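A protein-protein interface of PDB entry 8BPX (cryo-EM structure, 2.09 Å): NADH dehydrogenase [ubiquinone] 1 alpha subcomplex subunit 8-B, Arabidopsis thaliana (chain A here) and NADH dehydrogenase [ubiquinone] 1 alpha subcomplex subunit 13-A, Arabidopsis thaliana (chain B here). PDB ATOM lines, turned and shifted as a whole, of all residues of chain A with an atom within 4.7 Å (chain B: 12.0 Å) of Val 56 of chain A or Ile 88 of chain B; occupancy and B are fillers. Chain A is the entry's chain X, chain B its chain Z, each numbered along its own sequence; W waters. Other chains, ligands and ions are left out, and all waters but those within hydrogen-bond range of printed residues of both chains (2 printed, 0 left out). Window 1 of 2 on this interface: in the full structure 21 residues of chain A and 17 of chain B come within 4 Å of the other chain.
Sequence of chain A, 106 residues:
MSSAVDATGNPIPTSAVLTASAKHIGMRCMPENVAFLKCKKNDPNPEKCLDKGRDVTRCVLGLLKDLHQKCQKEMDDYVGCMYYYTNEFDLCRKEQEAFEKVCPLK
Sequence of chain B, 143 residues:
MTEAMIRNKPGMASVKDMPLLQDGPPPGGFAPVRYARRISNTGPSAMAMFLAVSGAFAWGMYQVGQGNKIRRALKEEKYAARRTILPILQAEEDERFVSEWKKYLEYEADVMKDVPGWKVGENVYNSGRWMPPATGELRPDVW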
ATOM      1  N   LEU A  18       4.007 -38.216 -23.339  1.00  0.00           N
ATOM      2  CA  LEU A  18       4.982 -37.132 -23.370  1.00  0.00           C
ATOM      3  C   LEU A  18       6.320 -37.606 -23.922  1.00  0.00           C
ATOM      4  O   LEU A  18       6.934 -36.925 -24.747  1.00  0.00           O
ATOM      5  CB  LEU A  18       5.148 -36.540 -21.971  1.00  0.00           C
ATOM      6  CG  LEU A  18       3.890 -35.874 -21.409  1.00  0.00           C
ATOM      7  CD1 LEU A  18       4.063 -35.530 -19.939  1.00  0.00           C
ATOM      8  CD2 LEU A  18       3.543 -34.638 -22.221  1.00  0.00           C
ATOM      9  N   GLU A  32       8.791 -21.368 -25.039  1.00  0.00           N
ATOM     10  CA  GLU A  32       8.169 -21.484 -23.725  1.00  0.00           C
ATOM     11  C   GLU A  32       9.045 -22.287 -22.772  1.00  0.00           C
ATOM     12  O   GLU A  32       9.200 -21.920 -21.599  1.00  0.00           O
ATOM     13  CB  GLU A  32       6.790 -22.131 -23.849  1.00  0.00           C
ATOM     14  CG  GLU A  32       5.722 -21.237 -24.444  1.00  0.00           C
ATOM     15  CD  GLU A  32       5.773 -21.195 -25.958  1.00  0.00           C
ATOM     16  OE1 GLU A  32       6.590 -21.928 -26.551  1.00  0.00           O
ATOM     17  OE2 GLU A  32       4.993 -20.423 -26.557  1.00  0.00           O
ATOM     18  N   ASN A  33       9.626 -23.385 -23.261  1.00  0.00           N
ATOM     19  CA  ASN A  33      10.510 -24.203 -22.437  1.00  0.00           C
ATOM     20  C   ASN A  33      11.698 -23.388 -21.939  1.00  0.00           C
ATOM     21  O   ASN A  33      12.019 -23.397 -20.744  1.00  0.00           O
ATOM     22  CB  ASN A  33      10.996 -25.416 -23.237  1.00  0.00           C
ATOM     23  CG  ASN A  33       9.991 -26.556 -23.252  1.00  0.00           C
ATOM     24  OD1 ASN A  33       8.966 -26.512 -22.575  1.00  0.00           O
ATOM     25  ND2 ASN A  33      10.284 -27.585 -24.036  1.00  0.00           N
ATOM     26  N   PHE A  36      10.627 -20.758 -19.326  1.00  0.00           N
ATOM     27  CA  PHE A  36      10.366 -21.403 -18.046  1.00  0.00           C
ATOM     28  C   PHE A  36      11.668 -21.757 -17.341  1.00  0.00           C
ATOM     29  O   PHE A  36      11.812 -21.545 -16.131  1.00  0.00           O
ATOM     30  CB  PHE A  36       9.515 -22.655 -18.262  1.00  0.00           C
ATOM     31  CG  PHE A  36       9.200 -23.404 -17.001  1.00  0.00           C
ATOM     32  CD1 PHE A  36       8.171 -22.995 -16.171  1.00  0.00           C
ATOM     33  CD2 PHE A  36       9.940 -24.522 -16.642  1.00  0.00           C
ATOM     34  CE1 PHE A  36       7.880 -23.690 -15.013  1.00  0.00           C
ATOM     35  CE2 PHE A  36       9.655 -25.215 -15.482  1.00  0.00           C
ATOM     36  CZ  PHE A  36       8.623 -24.797 -14.668  1.00  0.00           C
ATOM     37  N   LYS A  52       4.770 -18.697 -16.537  1.00  0.00           N
ATOM     38  CA  LYS A  52       5.557 -19.403 -17.541  1.00  0.00           C
ATOM     39  C   LYS A  52       5.173 -20.873 -17.601  1.00  0.00           C
ATOM     40  O   LYS A  52       5.162 -21.472 -18.685  1.00  0.00           O
ATOM     41  CB  LYS A  52       7.049 -19.248 -17.244  1.00  0.00           C
ATOM     42  CG  LYS A  52       7.717 -18.127 -18.014  1.00  0.00           C
ATOM     43  CD  LYS A  52       7.620 -16.815 -17.264  1.00  0.00           C
ATOM     44  CE  LYS A  52       8.191 -15.666 -18.078  1.00  0.00           C
ATOM     45  NZ  LYS A  52       9.654 -15.818 -18.302  1.00  0.00           N
ATOM     46  N   GLY A  53       4.836 -21.462 -16.453  1.00  0.00           N
ATOM     47  CA  GLY A  53       4.356 -22.832 -16.447  1.00  0.00           C
ATOM     48  C   GLY A  53       3.061 -23.000 -17.219  1.00  0.00           C
ATOM     49  O   GLY A  53       2.884 -23.981 -17.944  1.00  0.00           O
ATOM     50  N   ARG A  54       2.136 -22.048 -17.070  1.00  0.00           N
ATOM     51  CA  ARG A  54       0.891 -22.108 -17.830  1.00  0.00           C
ATOM     52  C   ARG A  54       1.154 -21.976 -19.326  1.00  0.00           C
ATOM     53  O   ARG A  54       0.529 -22.672 -20.136  1.00  0.00           O
ATOM     54  CB  ARG A  54      -0.077 -21.026 -17.351  1.00  0.00           C
ATOM     55  CG  ARG A  54      -0.624 -21.268 -15.953  1.00  0.00           C
ATOM     56  CD  ARG A  54      -1.672 -20.236 -15.565  1.00  0.00           C
ATOM     57  NE  ARG A  54      -1.083 -19.071 -14.915  1.00  0.00           N
ATOM     58  CZ  ARG A  54      -0.902 -18.953 -13.606  1.00  0.00           C
ATOM     59  NH1 ARG A  54      -1.251 -19.915 -12.771  1.00  0.00           N
ATOM     60  NH2 ARG A  54      -0.355 -17.839 -13.126  1.00  0.00           N
ATOM     61  N   ASP A  55       2.075 -21.090 -19.711  1.00  0.00           N
ATOM     62  CA  ASP A  55       2.449 -20.980 -21.123  1.00  0.00           C
ATOM     63  C   ASP A  55       2.986 -22.307 -21.655  1.00  0.00           C
ATOM     64  O   ASP A  55       2.573 -22.781 -22.727  1.00  0.00           O
ATOM     65  CB  ASP A  55       3.480 -19.866 -21.314  1.00  0.00           C
ATOM     66  CG  ASP A  55       3.006 -18.531 -20.771  1.00  0.00           C
ATOM     67  OD1 ASP A  55       3.678 -17.512 -21.033  1.00  0.00           O
ATOM     68  OD2 ASP A  55       1.953 -18.496 -20.102  1.00  0.00           O
ATOM     69  N   VAL A  56       3.896 -22.932 -20.901  1.00  0.00           N
ATOM     70  CA  VAL A  56       4.447 -24.223 -21.308  1.00  0.00           C
ATOM     71  C   VAL A  56       3.332 -25.253 -21.454  1.00  0.00           C
ATOM     72  O   VAL A  56       3.249 -25.972 -22.459  1.00  0.00           O
ATOM     73  CB  VAL A  56       5.514 -24.693 -20.301  1.00  0.00           C
ATOM     74  CG1 VAL A  56       5.648 -26.211 -20.327  1.00  0.00           C
ATOM     75  CG2 VAL A  56       6.853 -24.035 -20.582  1.00  0.00           C
ATOM     76  N   THR A  57       2.456 -25.334 -20.447  1.00  0.00           N
ATOM     77  CA  THR A  57       1.414 -26.353 -20.437  1.00  0.00           C
ATOM     78  C   THR A  57       0.455 -26.177 -21.603  1.00  0.00           C
ATOM     79  O   THR A  57       0.054 -27.157 -22.242  1.00  0.00           O
ATOM     80  CB  THR A  57       0.652 -26.307 -19.112  1.00  0.00           C
ATOM     81  OG1 THR A  57       1.574 -26.393 -18.019  1.00  0.00           O
ATOM     82  CG2 THR A  57      -0.340 -27.456 -19.025  1.00  0.00           C
ATOM     83  N   ARG A  58       0.072 -24.932 -21.895  1.00  0.00           N
ATOM     84  CA  ARG A  58      -0.826 -24.678 -23.014  1.00  0.00           C
ATOM     85  C   ARG A  58      -0.178 -25.063 -24.337  1.00  0.00           C
ATOM     86  O   ARG A  58      -0.812 -25.719 -25.174  1.00  0.00           O
ATOM     87  CB  ARG A  58      -1.242 -23.210 -23.011  1.00  0.00           C
ATOM     88  CG  ARG A  58      -1.673 -22.660 -24.347  1.00  0.00           C
ATOM     89  CD  ARG A  58      -2.138 -21.213 -24.223  1.00  0.00           C
ATOM     90  NE  ARG A  58      -2.622 -20.888 -22.886  1.00  0.00           N
ATOM     91  CZ  ARG A  58      -1.929 -20.216 -21.974  1.00  0.00           C
ATOM     92  NH1 ARG A  58      -0.708 -19.775 -22.220  1.00  0.00           N
ATOM     93  NH2 ARG A  58      -2.479 -19.981 -20.786  1.00  0.00           N
ATOM     94  N   CYS A  59       1.089 -24.682 -24.538  1.00  0.00           N
ATOM     95  CA  CYS A  59       1.784 -25.085 -25.759  1.00  0.00           C
ATOM     96  C   CYS A  59       1.790 -26.603 -25.912  1.00  0.00           C
ATOM     97  O   CYS A  59       1.459 -27.136 -26.981  1.00  0.00           O
ATOM     98  CB  CYS A  59       3.215 -24.544 -25.758  1.00  0.00           C
ATOM     99  SG  CYS A  59       4.180 -24.973 -27.230  1.00  0.00           S
ATOM    100  N   VAL A  60       2.148 -27.315 -24.841  1.00  0.00           N
ATOM    101  CA  VAL A  60       2.304 -28.764 -24.931  1.00  0.00           C
ATOM    102  C   VAL A  60       0.962 -29.439 -25.186  1.00  0.00           C
ATOM    103  O   VAL A  60       0.861 -30.349 -26.016  1.00  0.00           O
ATOM    104  CB  VAL A  60       2.982 -29.318 -23.665  1.00  0.00           C
ATOM    105  CG1 VAL A  60       3.065 -30.839 -23.738  1.00  0.00           C
ATOM    106  CG2 VAL A  60       4.364 -28.718 -23.497  1.00  0.00           C
ATOM    107  N   ALA B  80      17.916 -36.241 -24.082  1.00  0.00           N
ATOM    108  CA  ALA B  80      17.259 -35.128 -24.753  1.00  0.00           C
ATOM    109  C   ALA B  80      15.749 -35.240 -24.636  1.00  0.00           C
ATOM    110  O   ALA B  80      15.062 -34.238 -24.415  1.00  0.00           O
ATOM    111  CB  ALA B  80      17.681 -35.076 -26.221  1.00  0.00           C
ATOM    112  N   ALA B  81      15.211 -36.455 -24.783  1.00  0.00           N
ATOM    113  CA  ALA B  81      13.773 -36.631 -24.604  1.00  0.00           C
ATOM    114  C   ALA B  81      13.337 -36.186 -23.214  1.00  0.00           C
ATOM    115  O   ALA B  81      12.316 -35.508 -23.065  1.00  0.00           O
ATOM    116  CB  ALA B  81      13.380 -38.087 -24.846  1.00  0.00           C
ATOM    117  N   ARG B  82      14.109 -36.542 -22.187  1.00  0.00           N
ATOM    118  CA  ARG B  82      13.765 -36.089 -20.843  1.00  0.00           C
ATOM    119  C   ARG B  82      13.861 -34.574 -20.713  1.00  0.00           C
ATOM    120  O   ARG B  82      13.129 -33.970 -19.922  1.00  0.00           O
ATOM    121  CB  ARG B  82      14.658 -36.770 -19.811  1.00  0.00           C
ATOM    122  CG  ARG B  82      14.281 -38.211 -19.558  1.00  0.00           C
ATOM    123  CD  ARG B  82      15.358 -38.937 -18.792  1.00  0.00           C
ATOM    124  NE  ARG B  82      14.999 -40.328 -18.554  1.00  0.00           N
ATOM    125  CZ  ARG B  82      15.544 -41.089 -17.617  1.00  0.00           C
ATOM    126  NH1 ARG B  82      16.501 -40.631 -16.826  1.00  0.00           N
ATOM    127  NH2 ARG B  82      15.113 -42.337 -17.466  1.00  0.00           N
ATOM    128  N   ARG B  83      14.749 -33.943 -21.480  1.00  0.00           N
ATOM    129  CA  ARG B  83      14.953 -32.507 -21.345  1.00  0.00           C
ATOM    130  C   ARG B  83      13.800 -31.701 -21.938  1.00  0.00           C
ATOM    131  O   ARG B  83      13.451 -30.645 -21.402  1.00  0.00           O
ATOM    132  CB  ARG B  83      16.284 -32.114 -21.989  1.00  0.00           C
ATOM    133  CG  ARG B  83      17.453 -32.146 -21.015  1.00  0.00           C
ATOM    134  CD  ARG B  83      18.699 -31.491 -21.589  1.00  0.00           C
ATOM    135  NE  ARG B  83      19.197 -32.219 -22.748  1.00  0.00           N
ATOM    136  CZ  ARG B  83      20.152 -33.138 -22.705  1.00  0.00           C
ATOM    137  NH1 ARG B  83      20.774 -33.434 -21.579  1.00  0.00           N
ATOM    138  NH2 ARG B  83      20.488 -33.776 -23.822  1.00  0.00           N
ATOM    139  N   THR B  84      13.189 -32.180 -23.027  1.00  0.00           N
ATOM    140  CA  THR B  84      12.131 -31.404 -23.671  1.00  0.00           C
ATOM    141  C   THR B  84      10.820 -31.445 -22.895  1.00  0.00           C
ATOM    142  O   THR B  84      10.042 -30.489 -22.961  1.00  0.00           O
ATOM    143  CB  THR B  84      11.898 -31.880 -25.107  1.00  0.00           C
ATOM    144  OG1 THR B  84      11.030 -33.018 -25.110  1.00  0.00           O
ATOM    145  CG2 THR B  84      13.203 -32.222 -25.788  1.00  0.00           C
ATOM    146  N   ILE B  85      10.546 -32.530 -22.166  1.00  0.00           N
ATOM    147  CA  ILE B  85       9.319 -32.621 -21.377  1.00  0.00           C
ATOM    148  C   ILE B  85       9.529 -32.218 -19.928  1.00  0.00           C
ATOM    149  O   ILE B  85       8.578 -32.262 -19.137  1.00  0.00           O
ATOM    150  CB  ILE B  85       8.703 -34.032 -21.454  1.00  0.00           C
ATOM    151  CG1 ILE B  85       9.604 -35.060 -20.762  1.00  0.00           C
ATOM    152  CG2 ILE B  85       8.433 -34.417 -22.895  1.00  0.00           C
ATOM    153  CD1 ILE B  85       8.894 -36.338 -20.395  1.00  0.00           C
ATOM    154  N   LEU B  86      10.747 -31.828 -19.556  1.00  0.00           N
ATOM    155  CA  LEU B  86      11.003 -31.351 -18.199  1.00  0.00           C
ATOM    156  C   LEU B  86      10.122 -30.166 -17.807  1.00  0.00           C
ATOM    157  O   LEU B  86       9.538 -30.201 -16.708  1.00  0.00           O
ATOM    158  CB  LEU B  86      12.495 -31.015 -18.067  1.00  0.00           C
ATOM    159  CG  LEU B  86      13.097 -30.531 -16.746  1.00  0.00           C
ATOM    160  CD1 LEU B  86      12.968 -29.031 -16.567  1.00  0.00           C
ATOM    161  CD2 LEU B  86      12.456 -31.236 -15.605  1.00  0.00           C
ATOM    162  N   PRO B  87       9.996 -29.100 -18.611  1.00  0.00           N
ATOM    163  CA  PRO B  87       9.235 -27.929 -18.138  1.00  0.00           C
ATOM    164  C   PRO B  87       7.784 -28.213 -17.782  1.00  0.00           C
ATOM    165  O   PRO B  87       7.304 -27.683 -16.776  1.00  0.00           O
ATOM    166  CB  PRO B  87       9.353 -26.947 -19.312  1.00  0.00           C
ATOM    167  CG  PRO B  87      10.610 -27.332 -19.983  1.00  0.00           C
ATOM    168  CD  PRO B  87      10.657 -28.818 -19.899  1.00  0.00           C
ATOM    169  N   ILE B  88       7.072 -29.037 -18.553  1.00  0.00           N
ATOM    170  CA  ILE B  88       5.661 -29.269 -18.248  1.00  0.00           C
ATOM    171  C   ILE B  88       5.510 -30.091 -16.970  1.00  0.00           C
ATOM    172  O   ILE B  88       4.625 -29.826 -16.146  1.00  0.00           O
ATOM    173  CB  ILE B  88       4.937 -29.919 -19.444  1.00  0.00           C
ATOM    174  CG1 ILE B  88       3.433 -29.975 -19.165  1.00  0.00           C
ATOM    175  CG2 ILE B  88       5.499 -31.299 -19.771  1.00  0.00           C
ATOM    176  CD1 ILE B  88       2.637 -30.694 -20.211  1.00  0.00           C
ATOM    177  N   LEU B  89       6.381 -31.084 -16.771  1.00  0.00           N
ATOM    178  CA  LEU B  89       6.354 -31.844 -15.526  1.00  0.00           C
ATOM    179  C   LEU B  89       6.647 -30.945 -14.332  1.00  0.00           C
ATOM    180  O   LEU B  89       5.972 -31.032 -13.296  1.00  0.00           O
ATOM    181  CB  LEU B  89       7.356 -32.997 -15.600  1.00  0.00           C
ATOM    182  CG  LEU B  89       7.125 -33.993 -16.740  1.00  0.00           C
ATOM    183  CD1 LEU B  89       8.347 -34.878 -16.961  1.00  0.00           C
ATOM    184  CD2 LEU B  89       5.886 -34.840 -16.474  1.00  0.00           C
ATOM    185  N   GLN B  90       7.637 -30.059 -14.467  1.00  0.00           N
ATOM    186  CA  GLN B  90       7.961 -29.146 -13.377  1.00  0.00           C
ATOM    187  C   GLN B  90       6.811 -28.183 -13.099  1.00  0.00           C
ATOM    188  O   GLN B  90       6.532 -27.872 -11.941  1.00  0.00           O
ATOM    189  CB  GLN B  90       9.239 -28.372 -13.692  1.00  0.00           C
ATOM    190  CG  GLN B  90       9.981 -27.874 -12.464  1.00  0.00           C
ATOM    191  CD  GLN B  90       9.983 -28.876 -11.326  1.00  0.00           C
ATOM    192  OE1 GLN B  90      10.630 -29.917 -11.406  1.00  0.00           O
ATOM    193  NE2 GLN B  90       9.265 -28.562 -10.256  1.00  0.00           N
ATOM    194  N   ALA B  91       6.146 -27.692 -14.148  1.00  0.00           N
ATOM    195  CA  ALA B  91       5.025 -26.773 -13.956  1.00  0.00           C
ATOM    196  C   ALA B  91       3.868 -27.457 -13.239  1.00  0.00           C
ATOM    197  O   ALA B  91       3.253 -26.875 -12.334  1.00  0.00           O
ATOM    198  CB  ALA B  91       4.570 -26.222 -15.305  1.00  0.00           C
ATOM    199  N   GLU B  92       3.559 -28.694 -13.632  1.00  0.00           N
ATOM    200  CA  GLU B  92       2.553 -29.476 -12.924  1.00  0.00           C
ATOM    201  C   GLU B  92       2.922 -29.640 -11.454  1.00  0.00           C
ATOM    202  O   GLU B  92       2.084 -29.446 -10.562  1.00  0.00           O
ATOM    203  CB  GLU B  92       2.404 -30.839 -13.593  1.00  0.00           C
ATOM    204  CG  GLU B  92       1.349 -31.728 -12.987  1.00  0.00           C
ATOM    205  CD  GLU B  92       1.288 -33.077 -13.671  1.00  0.00           C
ATOM    206  OE1 GLU B  92       0.635 -33.178 -14.728  1.00  0.00           O
ATOM    207  OE2 GLU B  92       1.892 -34.036 -13.150  1.00  0.00           O
ATOM    208  N   GLU B  93       4.181 -29.996 -11.183  1.00  0.00           N
ATOM    209  CA  GLU B  93       4.612 -30.173  -9.802  1.00  0.00           C
ATOM    210  C   GLU B  93       4.520 -28.866  -9.023  1.00  0.00           C
ATOM    211  O   GLU B  93       4.158 -28.863  -7.842  1.00  0.00           O
ATOM    212  CB  GLU B  93       6.036 -30.732  -9.755  1.00  0.00           C
ATOM    213  CG  GLU B  93       6.677 -30.701  -8.372  1.00  0.00           C
ATOM    214  CD  GLU B  93       6.043 -31.667  -7.377  1.00  0.00           C
ATOM    215  OE1 GLU B  93       5.072 -32.369  -7.730  1.00  0.00           O
ATOM    216  OE2 GLU B  93       6.512 -31.709  -6.223  1.00  0.00           O
ATOM    217  N   ASP B  94       4.849 -27.745  -9.667  1.00  0.00           N
ATOM    218  CA  ASP B  94       4.776 -26.450  -8.998  1.00  0.00           C
ATOM    219  C   ASP B  94       3.341 -26.112  -8.620  1.00  0.00           C
ATOM    220  O   ASP B  94       3.072 -25.668  -7.499  1.00  0.00           O
ATOM    221  CB  ASP B  94       5.367 -25.363  -9.896  1.00  0.00           C
ATOM    222  CG  ASP B  94       6.883 -25.358  -9.889  1.00  0.00           C
ATOM    223  OD1 ASP B  94       7.480 -26.146  -9.126  1.00  0.00           O
ATOM    224  OD2 ASP B  94       7.475 -24.555 -10.638  1.00  0.00           O
ATOM    225  N   GLU B  95       2.401 -26.320  -9.545  1.00  0.00           N
ATOM    226  CA  GLU B  95       0.997 -26.065  -9.230  1.00  0.00           C
ATOM    227  C   GLU B  95       0.517 -26.957  -8.088  1.00  0.00           C
ATOM    228  O   GLU B  95      -0.147 -26.486  -7.150  1.00  0.00           O
ATOM    229  CB  GLU B  95       0.136 -26.272 -10.476  1.00  0.00           C
ATOM    230  CG  GLU B  95       0.185 -25.112 -11.459  1.00  0.00           C
ATOM    231  CD  GLU B  95      -0.766 -23.993 -11.094  1.00  0.00           C
ATOM    232  OE1 GLU B  95      -1.301 -24.004  -9.966  1.00  0.00           O
ATOM    233  OE2 GLU B  95      -0.986 -23.099 -11.938  1.00  0.00           O
ATOM    234  N   ARG B  96       0.870 -28.245  -8.139  1.00  0.00           N
ATOM    235  CA  ARG B  96       0.497 -29.167  -7.069  1.00  0.00           C
ATOM    236  C   ARG B  96       1.034 -28.704  -5.720  1.00  0.00           C
ATOM    237  O   ARG B  96       0.298 -28.656  -4.725  1.00  0.00           O
ATOM    238  CB  ARG B  96       1.007 -30.571  -7.398  1.00  0.00           C
ATOM    239  CG  ARG B  96       0.330 -31.678  -6.621  1.00  0.00           C
ATOM    240  CD  ARG B  96       1.260 -32.869  -6.430  1.00  0.00           C
ATOM    241  NE  ARG B  96       2.591 -32.473  -5.986  1.00  0.00           N
ATOM    242  CZ  ARG B  96       2.934 -32.279  -4.720  1.00  0.00           C
ATOM    243  NH1 ARG B  96       2.066 -32.438  -3.736  1.00  0.00           N
ATOM    244  NH2 ARG B  96       4.179 -31.912  -4.434  1.00  0.00           N
ATOM    245  N   PHE B  97       2.322 -28.353  -5.673  1.00  0.00           N
ATOM    246  CA  PHE B  97       2.923 -27.942  -4.412  1.00  0.00           C
ATOM    247  C   PHE B  97       2.316 -26.644  -3.901  1.00  0.00           C
ATOM    248  O   PHE B  97       2.146 -26.476  -2.693  1.00  0.00           O
ATOM    249  CB  PHE B  97       4.435 -27.786  -4.548  1.00  0.00           C
ATOM    250  CG  PHE B  97       5.096 -27.328  -3.283  1.00  0.00           C
ATOM    251  CD1 PHE B  97       5.438 -28.238  -2.299  1.00  0.00           C
ATOM    252  CD2 PHE B  97       5.339 -25.984  -3.058  1.00  0.00           C
ATOM    253  CE1 PHE B  97       6.032 -27.820  -1.126  1.00  0.00           C
ATOM    254  CE2 PHE B  97       5.926 -25.561  -1.884  1.00  0.00           C
ATOM    255  CZ  PHE B  97       6.277 -26.481  -0.920  1.00  0.00           C
HETATM  256  O   HOH W   1       7.664 -29.381 -21.597  1.00  0.00           O
HETATM  257  O   HOH W   2       2.108 -28.459 -16.330  1.00  0.00           O
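Hydrophobic or aromatic side chains of chain B within 4 Å of the printed part of chain A: Ile 85, Pro 87, Ile 88, Leu 89 and Ala 91.
Leu 18 of chain A touches Ile 85 of chain B (O to CG2, 3.5 Å).
Leu 18 of chain A touches Leu 89 of chain B (CD1 to CD2, 3.98 Å).
Asn 33 of chain A touches Pro 87 of chain B.
Pro 87 of chain B touches Phe 36 of chain A (O to CE2, 3.6 Å).
CB of Gln 90 of chain B touches CE2 of Phe 36 of chain A, 3.7 Å away.
Phe 36 of chain A touches Ala 91 of chain B (CZ to N, 3.8 Å).
Gly 53 of chain A touches Ala 91 of chain B (CA to CB, 3.6 Å).
Pro 87 of chain B touches Val 56 of chain A (C to CG1, 3.9 Å).
CG1 of Val 56 of chain A touches N of Ile 88 of chain B (3.6 Å).
Ile 88 of chain B touches Val 60 of chain A (CD1 to CG1, 3.6 Å).
Water W2 lies within hydrogen-bond range of OG1 of Thr 57 of chain A (2.7 Å), O of Ile 88 of chain B (2.9 Å) and N of Glu 92 of chain B (3.1 Å).
Water W1 lies within hydrogen-bond range of the backbone carbonyl oxygen (O) of Thr 84 of chain B (3.0 Å), the backbone NH (N) of Ile 88 of chain B (3.1 Å) and the side-chain amide oxygen (OD1) of Asn 33 of chain A (3.3 Å).
The side-chain amide nitrogen of Asn 33 of chain A is in hydrogen-bond range of the backbone carbonyl oxygen of Thr 84 of chain B, 3.1 Å away.
The guanidinium group of Arg 54 of chain A lies within salt-bridge range of the side-chain carboxylate of Glu 95 of chain B (3.3 Å).
The backbone carbonyl oxygen (O) of Gly 53 of chain A sits at hydrogen-bond distance from the side-chain hydroxyl (OG1) of Thr 57 of chain A.
The backbone carbonyl oxygen of Ala 81 of chain B lies within hydrogen-bond range of the side-chain hydroxyl of Thr 84 of chain B, at 3.5 Å.
The side-chain amide nitrogen (NE2) of Gln 90 of chain B sits at hydrogen-bond distance from the side-chain carboxylate (OD1) of Asp 94 of chain B, 3.2 Å away.
Leu 18 of chain A touches two residues of chain B.
No residue of chain B comes within 4 Å of Glu 32 of chain A.
Asn 33 of chain A touches just these residues of chain B: Thr 84 and Pro 87.
Lys 52 of chain A touches none of the printed residues of chain B.
Printed residues of chain B within 4 Å of Arg 54 of chain A: Glu 95 (3.3 Å).
Thr 57 of chain A touches none of the printed residues of chain B.
No residue of chain B comes within 4 Å of Cys 59 of chain A.
Ala 80 of chain B touches none of the printed residues of chain A.
Ile 88 of chain B touches two residues of chain A.
Printed residues of chain A within 4 Å of Leu 89 of chain B: Leu 18 (3.98 Å).
The nearest residue of chain B that does not touch Val 56 of chain A is Ala 91 of chain B (5.1 Å).
The nearest residue of chain A that does not touch Ile 88 of chain B is Thr 57 of chain A (4.2 Å).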
